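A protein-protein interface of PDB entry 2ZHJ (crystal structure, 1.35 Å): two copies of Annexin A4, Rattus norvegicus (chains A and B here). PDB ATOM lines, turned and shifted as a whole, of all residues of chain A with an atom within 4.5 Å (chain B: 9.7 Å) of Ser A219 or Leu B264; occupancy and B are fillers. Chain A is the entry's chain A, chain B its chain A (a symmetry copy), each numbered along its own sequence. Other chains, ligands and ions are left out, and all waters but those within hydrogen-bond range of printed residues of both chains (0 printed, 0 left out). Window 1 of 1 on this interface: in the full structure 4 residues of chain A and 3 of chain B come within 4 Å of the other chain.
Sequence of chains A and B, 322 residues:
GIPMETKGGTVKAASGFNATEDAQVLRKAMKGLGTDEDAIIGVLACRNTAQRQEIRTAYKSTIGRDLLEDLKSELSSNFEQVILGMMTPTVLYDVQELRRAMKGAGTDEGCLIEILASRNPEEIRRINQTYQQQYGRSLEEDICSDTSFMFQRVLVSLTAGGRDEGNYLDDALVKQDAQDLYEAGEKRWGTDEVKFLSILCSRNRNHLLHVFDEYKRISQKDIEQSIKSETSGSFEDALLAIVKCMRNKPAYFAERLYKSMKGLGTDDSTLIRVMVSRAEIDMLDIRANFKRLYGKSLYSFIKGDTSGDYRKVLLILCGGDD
N of Lys A221 sits at hydrogen-bond distance from OG of Ser A219, at 3.0 Å.
The side-chain hydroxyl of Ser A219 lies within hydrogen-bond range of the backbone carbonyl oxygen of Tyr A215.
The side-chain amino group of Lys A216 is in hydrogen-bond range of the backbone carbonyl oxygen of Gln A220 (3.0 Å).
O of Arg A217 lies within hydrogen-bond range of NE2 of Gln A220 (3.3 Å).
Of the 12 printed residues of chain B, 3 touch a printed residue of chain A.
Printed residues of chain B that touch a printed residue of chain A: Lys B262, Gly B263 and Leu B264.
Along chain B the printed residues that touch a printed residue of chain A span positions 262 to 264.
Of the 9 printed residues of chain A, 4 touch a printed residue of chain B.
Printed residues of chain A that touch a printed residue of chain B: Tyr A182, Glu A186, Ser A219 and Gln A220.
Hydrophobic or aromatic side chains of chain A within 4 Å of the printed part of chain B: Tyr A182.
Among the printed residues, no Asp or Glu carboxylate lies within 4 Å of a Lys or Arg side-chain nitrogen of the other chain.
No position is printed for both chains.
Of the 7 pairs that touch across the chains among the printed residues, none has its exchanged pair printed and touching as well.
Printed residues of chain B within 4 Å of Tyr A182: Gly B263 and Leu B264.
Printed residues of chain B within 4 Å of Glu A186: Leu B264 (2.8 Å).
No residue of chain B comes within 4 Å of Ile A218.
Printed residues of chain B within 4 Å of Ser A219: Gly B263 (3.8 Å) and Leu B264 (3.7 Å).
Printed residues of chain B within 4 Å of Gln A220: Lys B262 and Gly B263.
Printed residues of chain A within 4 Å of Lys B262: Gln A220.
Printed residues of chain A within 4 Å of Gly B263: Tyr A182, Ser A219 and Gln A220.
Thr B266 touches none of the printed residues of chain A.
The nearest residue of chain B that does not touch Ser A219 is Lys B262 (5.4 Å).
The nearest printed residue of chain A that does not touch Gly B263 is Ile A218 (4.7 Å).
Gly B263 touches Tyr A182.
OE1 of Glu A186 touches CD2 of Leu B264 (2.8 Å).
Gly B263 touches Ser A219.
N of Leu B264 touches O of Ser A219, at 3.7 Å.
Lys B262 touches Gln A220.
CA of Gly B263 touches CG of Gln A220 (3.4 Å).
The side-chain hydroxyl (OH) of Tyr A182 is in hydrogen-bond range of the backbone NH (N) of Leu B264 (3.1 Å).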
ATOM      1  N   TYR A 182     -11.919 -17.107  24.388  1.00  0.00           N
ATOM      2  CA  TYR A 182     -11.294 -15.972  25.088  1.00  0.00           C
ATOM      3  C   TYR A 182      -9.904 -16.373  25.532  1.00  0.00           C
ATOM      4  O   TYR A 182      -8.937 -15.627  25.297  1.00  0.00           O
ATOM      5  CB  TYR A 182     -12.148 -15.519  26.272  1.00  0.00           C
ATOM      6  CG  TYR A 182     -11.875 -14.156  26.858  1.00  0.00           C
ATOM      7  CD1 TYR A 182     -11.458 -13.078  26.093  1.00  0.00           C
ATOM      8  CD2 TYR A 182     -12.051 -13.948  28.242  1.00  0.00           C
ATOM      9  CE1 TYR A 182     -11.224 -11.841  26.707  1.00  0.00           C
ATOM     10  CE2 TYR A 182     -11.824 -12.740  28.839  1.00  0.00           C
ATOM     11  CZ  TYR A 182     -11.410 -11.680  28.059  1.00  0.00           C
ATOM     12  OH  TYR A 182     -11.171 -10.441  28.650  1.00  0.00           O
ATOM     13  N   GLU A 186      -7.548 -13.525  23.146  1.00  0.00           N
ATOM     14  CA  GLU A 186      -7.366 -12.271  23.858  1.00  0.00           C
ATOM     15  C   GLU A 186      -6.639 -12.500  25.179  1.00  0.00           C
ATOM     16  O   GLU A 186      -5.805 -11.645  25.465  1.00  0.00           O
ATOM     17  CB  GLU A 186      -8.698 -11.563  24.181  1.00  0.00           C
ATOM     18  CG  GLU A 186      -9.464 -11.175  22.922  1.00  0.00           C
ATOM     19  CD  GLU A 186      -9.102  -9.825  22.369  1.00  0.00           C
ATOM     20  OE1 GLU A 186      -8.180  -9.139  22.870  1.00  0.00           O
ATOM     21  OE2 GLU A 186      -9.801  -9.444  21.409  1.00  0.00           O
ATOM     22  N   TYR A 215     -19.510 -14.841  24.321  1.00  0.00           N
ATOM     23  CA  TYR A 215     -18.162 -14.292  24.145  1.00  0.00           C
ATOM     24  C   TYR A 215     -18.190 -12.794  24.391  1.00  0.00           C
ATOM     25  O   TYR A 215     -17.305 -12.213  25.014  1.00  0.00           O
ATOM     26  CB  TYR A 215     -17.638 -14.620  22.731  1.00  0.00           C
ATOM     27  CG  TYR A 215     -16.218 -14.118  22.582  1.00  0.00           C
ATOM     28  CD1 TYR A 215     -15.899 -12.886  22.056  1.00  0.00           C
ATOM     29  CD2 TYR A 215     -15.185 -14.954  23.018  1.00  0.00           C
ATOM     30  CE1 TYR A 215     -14.612 -12.446  21.939  1.00  0.00           C
ATOM     31  CE2 TYR A 215     -13.875 -14.513  22.895  1.00  0.00           C
ATOM     32  CZ  TYR A 215     -13.612 -13.283  22.359  1.00  0.00           C
ATOM     33  OH  TYR A 215     -12.312 -12.869  22.261  1.00  0.00           O
ATOM     34  N   LYS A 216     -19.200 -12.105  23.878  1.00  0.00           N
ATOM     35  CA  LYS A 216     -19.280 -10.654  24.113  1.00  0.00           C
ATOM     36  C   LYS A 216     -19.454 -10.319  25.587  1.00  0.00           C
ATOM     37  O   LYS A 216     -18.819  -9.363  26.095  1.00  0.00           O
ATOM     38  CB  LYS A 216     -20.420 -10.115  23.248  1.00  0.00           C
ATOM     39  CG  LYS A 216     -20.794  -8.666  23.456  1.00  0.00           C
ATOM     40  CD  LYS A 216     -19.690  -7.706  23.052  1.00  0.00           C
ATOM     41  CE  LYS A 216     -19.918  -6.373  23.739  1.00  0.00           C
ATOM     42  NZ  LYS A 216     -19.281  -5.243  23.018  1.00  0.00           N
ATOM     43  N   ARG A 217     -20.292 -11.084  26.269  1.00  0.00           N
ATOM     44  CA  ARG A 217     -20.534 -10.888  27.695  1.00  0.00           C
ATOM     45  C   ARG A 217     -19.247 -11.016  28.496  1.00  0.00           C
ATOM     46  O   ARG A 217     -18.975 -10.258  29.414  1.00  0.00           O
ATOM     47  CB  ARG A 217     -21.604 -11.886  28.199  1.00  0.00           C
ATOM     48  CG  ARG A 217     -21.746 -11.914  29.698  1.00  0.00           C
ATOM     49  CD  ARG A 217     -22.821 -12.851  30.242  1.00  0.00           C
ATOM     50  NE  ARG A 217     -22.256 -14.061  30.828  1.00  0.00           N
ATOM     51  CZ  ARG A 217     -21.618 -14.209  31.972  1.00  0.00           C
ATOM     52  NH1 ARG A 217     -21.437 -13.157  32.758  1.00  0.00           N
ATOM     53  NH2 ARG A 217     -21.165 -15.401  32.339  1.00  0.00           N
ATOM     54  N   ILE A 218     -18.391 -11.976  28.192  1.00  0.00           N
ATOM     55  CA  ILE A 218     -17.214 -12.216  29.041  1.00  0.00           C
ATOM     56  C   ILE A 218     -15.986 -11.427  28.631  1.00  0.00           C
ATOM     57  O   ILE A 218     -15.112 -11.271  29.514  1.00  0.00           O
ATOM     58  CB  ILE A 218     -16.884 -13.713  29.059  1.00  0.00           C
ATOM     59  CG1 ILE A 218     -16.341 -14.263  27.740  1.00  0.00           C
ATOM     60  CG2 ILE A 218     -18.111 -14.494  29.510  1.00  0.00           C
ATOM     61  CD1 ILE A 218     -15.886 -15.714  27.858  1.00  0.00           C
ATOM     62  N   SER A 219     -15.959 -10.927  27.389  1.00  0.00           N
ATOM     63  CA  SER A 219     -14.774 -10.185  26.955  1.00  0.00           C
ATOM     64  C   SER A 219     -14.938  -8.699  26.695  1.00  0.00           C
ATOM     65  O   SER A 219     -13.961  -7.940  26.614  1.00  0.00           O
ATOM     66  CB  SER A 219     -14.279 -10.848  25.654  1.00  0.00           C
ATOM     67  OG  SER A 219     -15.064 -10.452  24.555  1.00  0.00           O
ATOM     68  N   GLN A 220     -16.158  -8.229  26.576  1.00  0.00           N
ATOM     69  CA  GLN A 220     -16.517  -6.885  26.139  1.00  0.00           C
ATOM     70  C   GLN A 220     -16.292  -6.631  24.642  1.00  0.00           C
ATOM     71  O   GLN A 220     -16.484  -5.498  24.166  1.00  0.00           O
ATOM     72  CB  GLN A 220     -15.767  -5.836  26.972  1.00  0.00           C
ATOM     73  CG  GLN A 220     -15.794  -6.078  28.478  1.00  0.00           C
ATOM     74  CD  GLN A 220     -17.213  -6.212  28.987  1.00  0.00           C
ATOM     75  OE1 GLN A 220     -17.990  -5.275  28.775  1.00  0.00           O
ATOM     76  NE2 GLN A 220     -17.515  -7.341  29.625  1.00  0.00           N
ATOM     77  N   LYS A 221     -15.898  -7.678  23.900  1.00  0.00           N
ATOM     78  CA  LYS A 221     -15.645  -7.567  22.481  1.00  0.00           C
ATOM     79  C   LYS A 221     -16.514  -8.562  21.711  1.00  0.00           C
ATOM     80  O   LYS A 221     -16.780  -9.688  22.205  1.00  0.00           O
ATOM     81  CB  LYS A 221     -14.191  -7.860  22.092  1.00  0.00           C
ATOM     82  CG  LYS A 221     -13.139  -6.967  22.715  1.00  0.00           C
ATOM     83  CD  LYS A 221     -13.032  -5.604  22.081  1.00  0.00           C
ATOM     84  CE  LYS A 221     -12.068  -4.703  22.861  1.00  0.00           C
ATOM     85  NZ  LYS A 221     -12.542  -3.284  22.884  1.00  0.00           N
ATOM     86  N   TYR B 258     -15.783   1.594  35.683  1.00  0.00           N
ATOM     87  CA  TYR B 258     -16.146   0.242  35.243  1.00  0.00           C
ATOM     88  C   TYR B 258     -15.609  -0.008  33.856  1.00  0.00           C
ATOM     89  O   TYR B 258     -15.008  -1.053  33.576  1.00  0.00           O
ATOM     90  CB  TYR B 258     -17.680   0.179  35.262  1.00  0.00           C
ATOM     91  CG  TYR B 258     -18.250  -1.141  34.768  1.00  0.00           C
ATOM     92  CD1 TYR B 258     -18.392  -2.251  35.584  1.00  0.00           C
ATOM     93  CD2 TYR B 258     -18.660  -1.267  33.439  1.00  0.00           C
ATOM     94  CE1 TYR B 258     -18.914  -3.439  35.107  1.00  0.00           C
ATOM     95  CE2 TYR B 258     -19.182  -2.453  32.968  1.00  0.00           C
ATOM     96  CZ  TYR B 258     -19.312  -3.536  33.801  1.00  0.00           C
ATOM     97  OH  TYR B 258     -19.841  -4.727  33.306  1.00  0.00           O
ATOM     98  N   LYS B 259     -15.827   0.934  32.941  1.00  0.00           N
ATOM     99  CA  LYS B 259     -15.400   0.659  31.553  1.00  0.00           C
ATOM    100  C   LYS B 259     -13.892   0.626  31.442  1.00  0.00           C
ATOM    101  O   LYS B 259     -13.337  -0.078  30.567  1.00  0.00           O
ATOM    102  CB  LYS B 259     -16.059   1.724  30.662  1.00  0.00           C
ATOM    103  CG  LYS B 259     -17.587   1.558  30.589  1.00  0.00           C
ATOM    104  CD  LYS B 259     -18.187   2.531  29.554  1.00  0.00           C
ATOM    105  CE  LYS B 259     -19.696   2.442  29.467  1.00  0.00           C
ATOM    106  NZ  LYS B 259     -20.282   2.802  28.154  1.00  0.00           N
ATOM    107  N   SER B 260     -13.188   1.316  32.347  1.00  0.00           N
ATOM    108  CA  SER B 260     -11.714   1.259  32.277  1.00  0.00           C
ATOM    109  C   SER B 260     -11.143  -0.089  32.690  1.00  0.00           C
ATOM    110  O   SER B 260     -10.001  -0.435  32.358  1.00  0.00           O
ATOM    111  CB  SER B 260     -11.120   2.398  33.144  1.00  0.00           C
ATOM    112  OG  SER B 260     -11.158   2.086  34.554  1.00  0.00           O
ATOM    113  N   MET B 261     -11.891  -0.891  33.448  1.00  0.00           N
ATOM    114  CA  MET B 261     -11.426  -2.149  34.024  1.00  0.00           C
ATOM    115  C   MET B 261     -12.148  -3.372  33.507  1.00  0.00           C
ATOM    116  O   MET B 261     -11.445  -4.411  33.439  1.00  0.00           O
ATOM    117  CB  MET B 261     -11.570  -2.160  35.577  1.00  0.00           C
ATOM    118  CG  MET B 261     -10.546  -1.172  36.190  1.00  0.00           C
ATOM    119  SD  MET B 261     -10.697  -1.079  37.983  1.00  0.00           S
ATOM    120  CE  MET B 261     -12.059   0.056  38.207  1.00  0.00           C
ATOM    121  N   LYS B 262     -13.428  -3.307  33.183  1.00  0.00           N
ATOM    122  CA  LYS B 262     -14.202  -4.482  32.759  1.00  0.00           C
ATOM    123  C   LYS B 262     -13.685  -5.032  31.428  1.00  0.00           C
ATOM    124  O   LYS B 262     -13.370  -4.285  30.516  1.00  0.00           O
ATOM    125  CB  LYS B 262     -15.709  -4.187  32.659  1.00  0.00           C
ATOM    126  CG  LYS B 262     -16.526  -5.450  32.359  1.00  0.00           C
ATOM    127  CD  LYS B 262     -16.764  -6.368  33.543  1.00  0.00           C
ATOM    128  CE  LYS B 262     -17.838  -7.390  33.291  1.00  0.00           C
ATOM    129  NZ  LYS B 262     -18.030  -8.347  34.419  1.00  0.00           N
ATOM    130  N   GLY B 263     -13.637  -6.364  31.368  1.00  0.00           N
ATOM    131  CA  GLY B 263     -13.079  -7.097  30.237  1.00  0.00           C
ATOM    132  C   GLY B 263     -11.573  -6.991  30.125  1.00  0.00           C
ATOM    133  O   GLY B 263     -10.771  -6.673  30.995  1.00  0.00           O
ATOM    134  N   LEU B 264     -11.108  -7.327  28.918  1.00  0.00           N
ATOM    135  CA  LEU B 264      -9.687  -7.445  28.706  1.00  0.00           C
ATOM    136  C   LEU B 264      -9.039  -6.066  28.795  1.00  0.00           C
ATOM    137  O   LEU B 264      -9.562  -5.116  28.216  1.00  0.00           O
ATOM    138  CB  LEU B 264      -9.384  -8.032  27.334  1.00  0.00           C
ATOM    139  CG  LEU B 264      -7.886  -8.252  27.052  1.00  0.00           C
ATOM    140  CD1 LEU B 264      -7.304  -9.242  28.043  1.00  0.00           C
ATOM    141  CD2 LEU B 264      -7.678  -8.701  25.622  1.00  0.00           C
ATOM    142  N   GLY B 265      -7.935  -6.100  29.519  1.00  0.00           N
ATOM    143  CA  GLY B 265      -7.080  -4.955  29.708  1.00  0.00           C
ATOM    144  C   GLY B 265      -7.528  -3.973  30.758  1.00  0.00           C
ATOM    145  O   GLY B 265      -8.574  -4.093  31.393  1.00  0.00           O
ATOM    146  N   THR B 266      -6.713  -2.959  30.974  1.00  0.00           N
ATOM    147  CA  THR B 266      -7.088  -1.855  31.842  1.00  0.00           C
ATOM    148  C   THR B 266      -6.702  -0.558  31.138  1.00  0.00           C
ATOM    149  O   THR B 266      -5.575  -0.458  30.653  1.00  0.00           O
ATOM    150  CB  THR B 266      -6.384  -1.846  33.208  1.00  0.00           C
ATOM    151  OG1 THR B 266      -6.576  -3.124  33.815  1.00  0.00           O
ATOM    152  CG2 THR B 266      -6.936  -0.735  34.103  1.00  0.00           C
ATOM    153  N   ASP B 267      -7.629   0.367  31.151  1.00  0.00           N
ATOM    154  CA  ASP B 267      -7.311   1.719  30.646  1.00  0.00           C
ATOM    155  C   ASP B 267      -6.764   2.464  31.852  1.00  0.00           C
ATOM    156  O   ASP B 267      -7.481   3.179  32.560  1.00  0.00           O
ATOM    157  CB  ASP B 267      -8.545   2.360  30.062  1.00  0.00           C
ATOM    158  CG  ASP B 267      -8.353   3.798  29.642  1.00  0.00           C
ATOM    159  OD1 ASP B 267      -7.208   4.305  29.736  1.00  0.00           O
ATOM    160  OD2 ASP B 267      -9.345   4.424  29.234  1.00  0.00           O
ATOM    161  N   ASP B 268      -5.463   2.301  32.105  1.00  0.00           N
ATOM    162  CA  ASP B 268      -4.856   2.902  33.294  1.00  0.00           C
ATOM    163  C   ASP B 268      -4.944   4.404  33.265  1.00  0.00           C
ATOM    164  O   ASP B 268      -5.092   5.031  34.320  1.00  0.00           O
ATOM    165  CB  ASP B 268      -3.392   2.430  33.367  1.00  0.00           C
ATOM    166  CG  ASP B 268      -3.273   0.944  33.667  1.00  0.00           C
ATOM    167  OD1 ASP B 268      -3.712   0.445  34.714  1.00  0.00           O
ATOM    168  OD2 ASP B 268      -2.747   0.209  32.794  1.00  0.00           O
ATOM    169  N   ASP B 305      -7.960  -5.960  39.368  1.00  0.00           N
ATOM    170  CA  ASP B 305      -7.437  -5.554  38.060  1.00  0.00           C
ATOM    171  C   ASP B 305      -6.101  -4.827  38.089  1.00  0.00           C
ATOM    172  O   ASP B 305      -5.621  -4.454  37.009  1.00  0.00           O
ATOM    173  CB  ASP B 305      -8.479  -4.625  37.396  1.00  0.00           C
ATOM    174  CG  ASP B 305      -8.456  -4.660  35.895  1.00  0.00           C
ATOM    175  OD1 ASP B 305      -8.343  -5.729  35.318  1.00  0.00           O
ATOM    176  OD2 ASP B 305      -8.575  -3.586  35.283  1.00  0.00           O
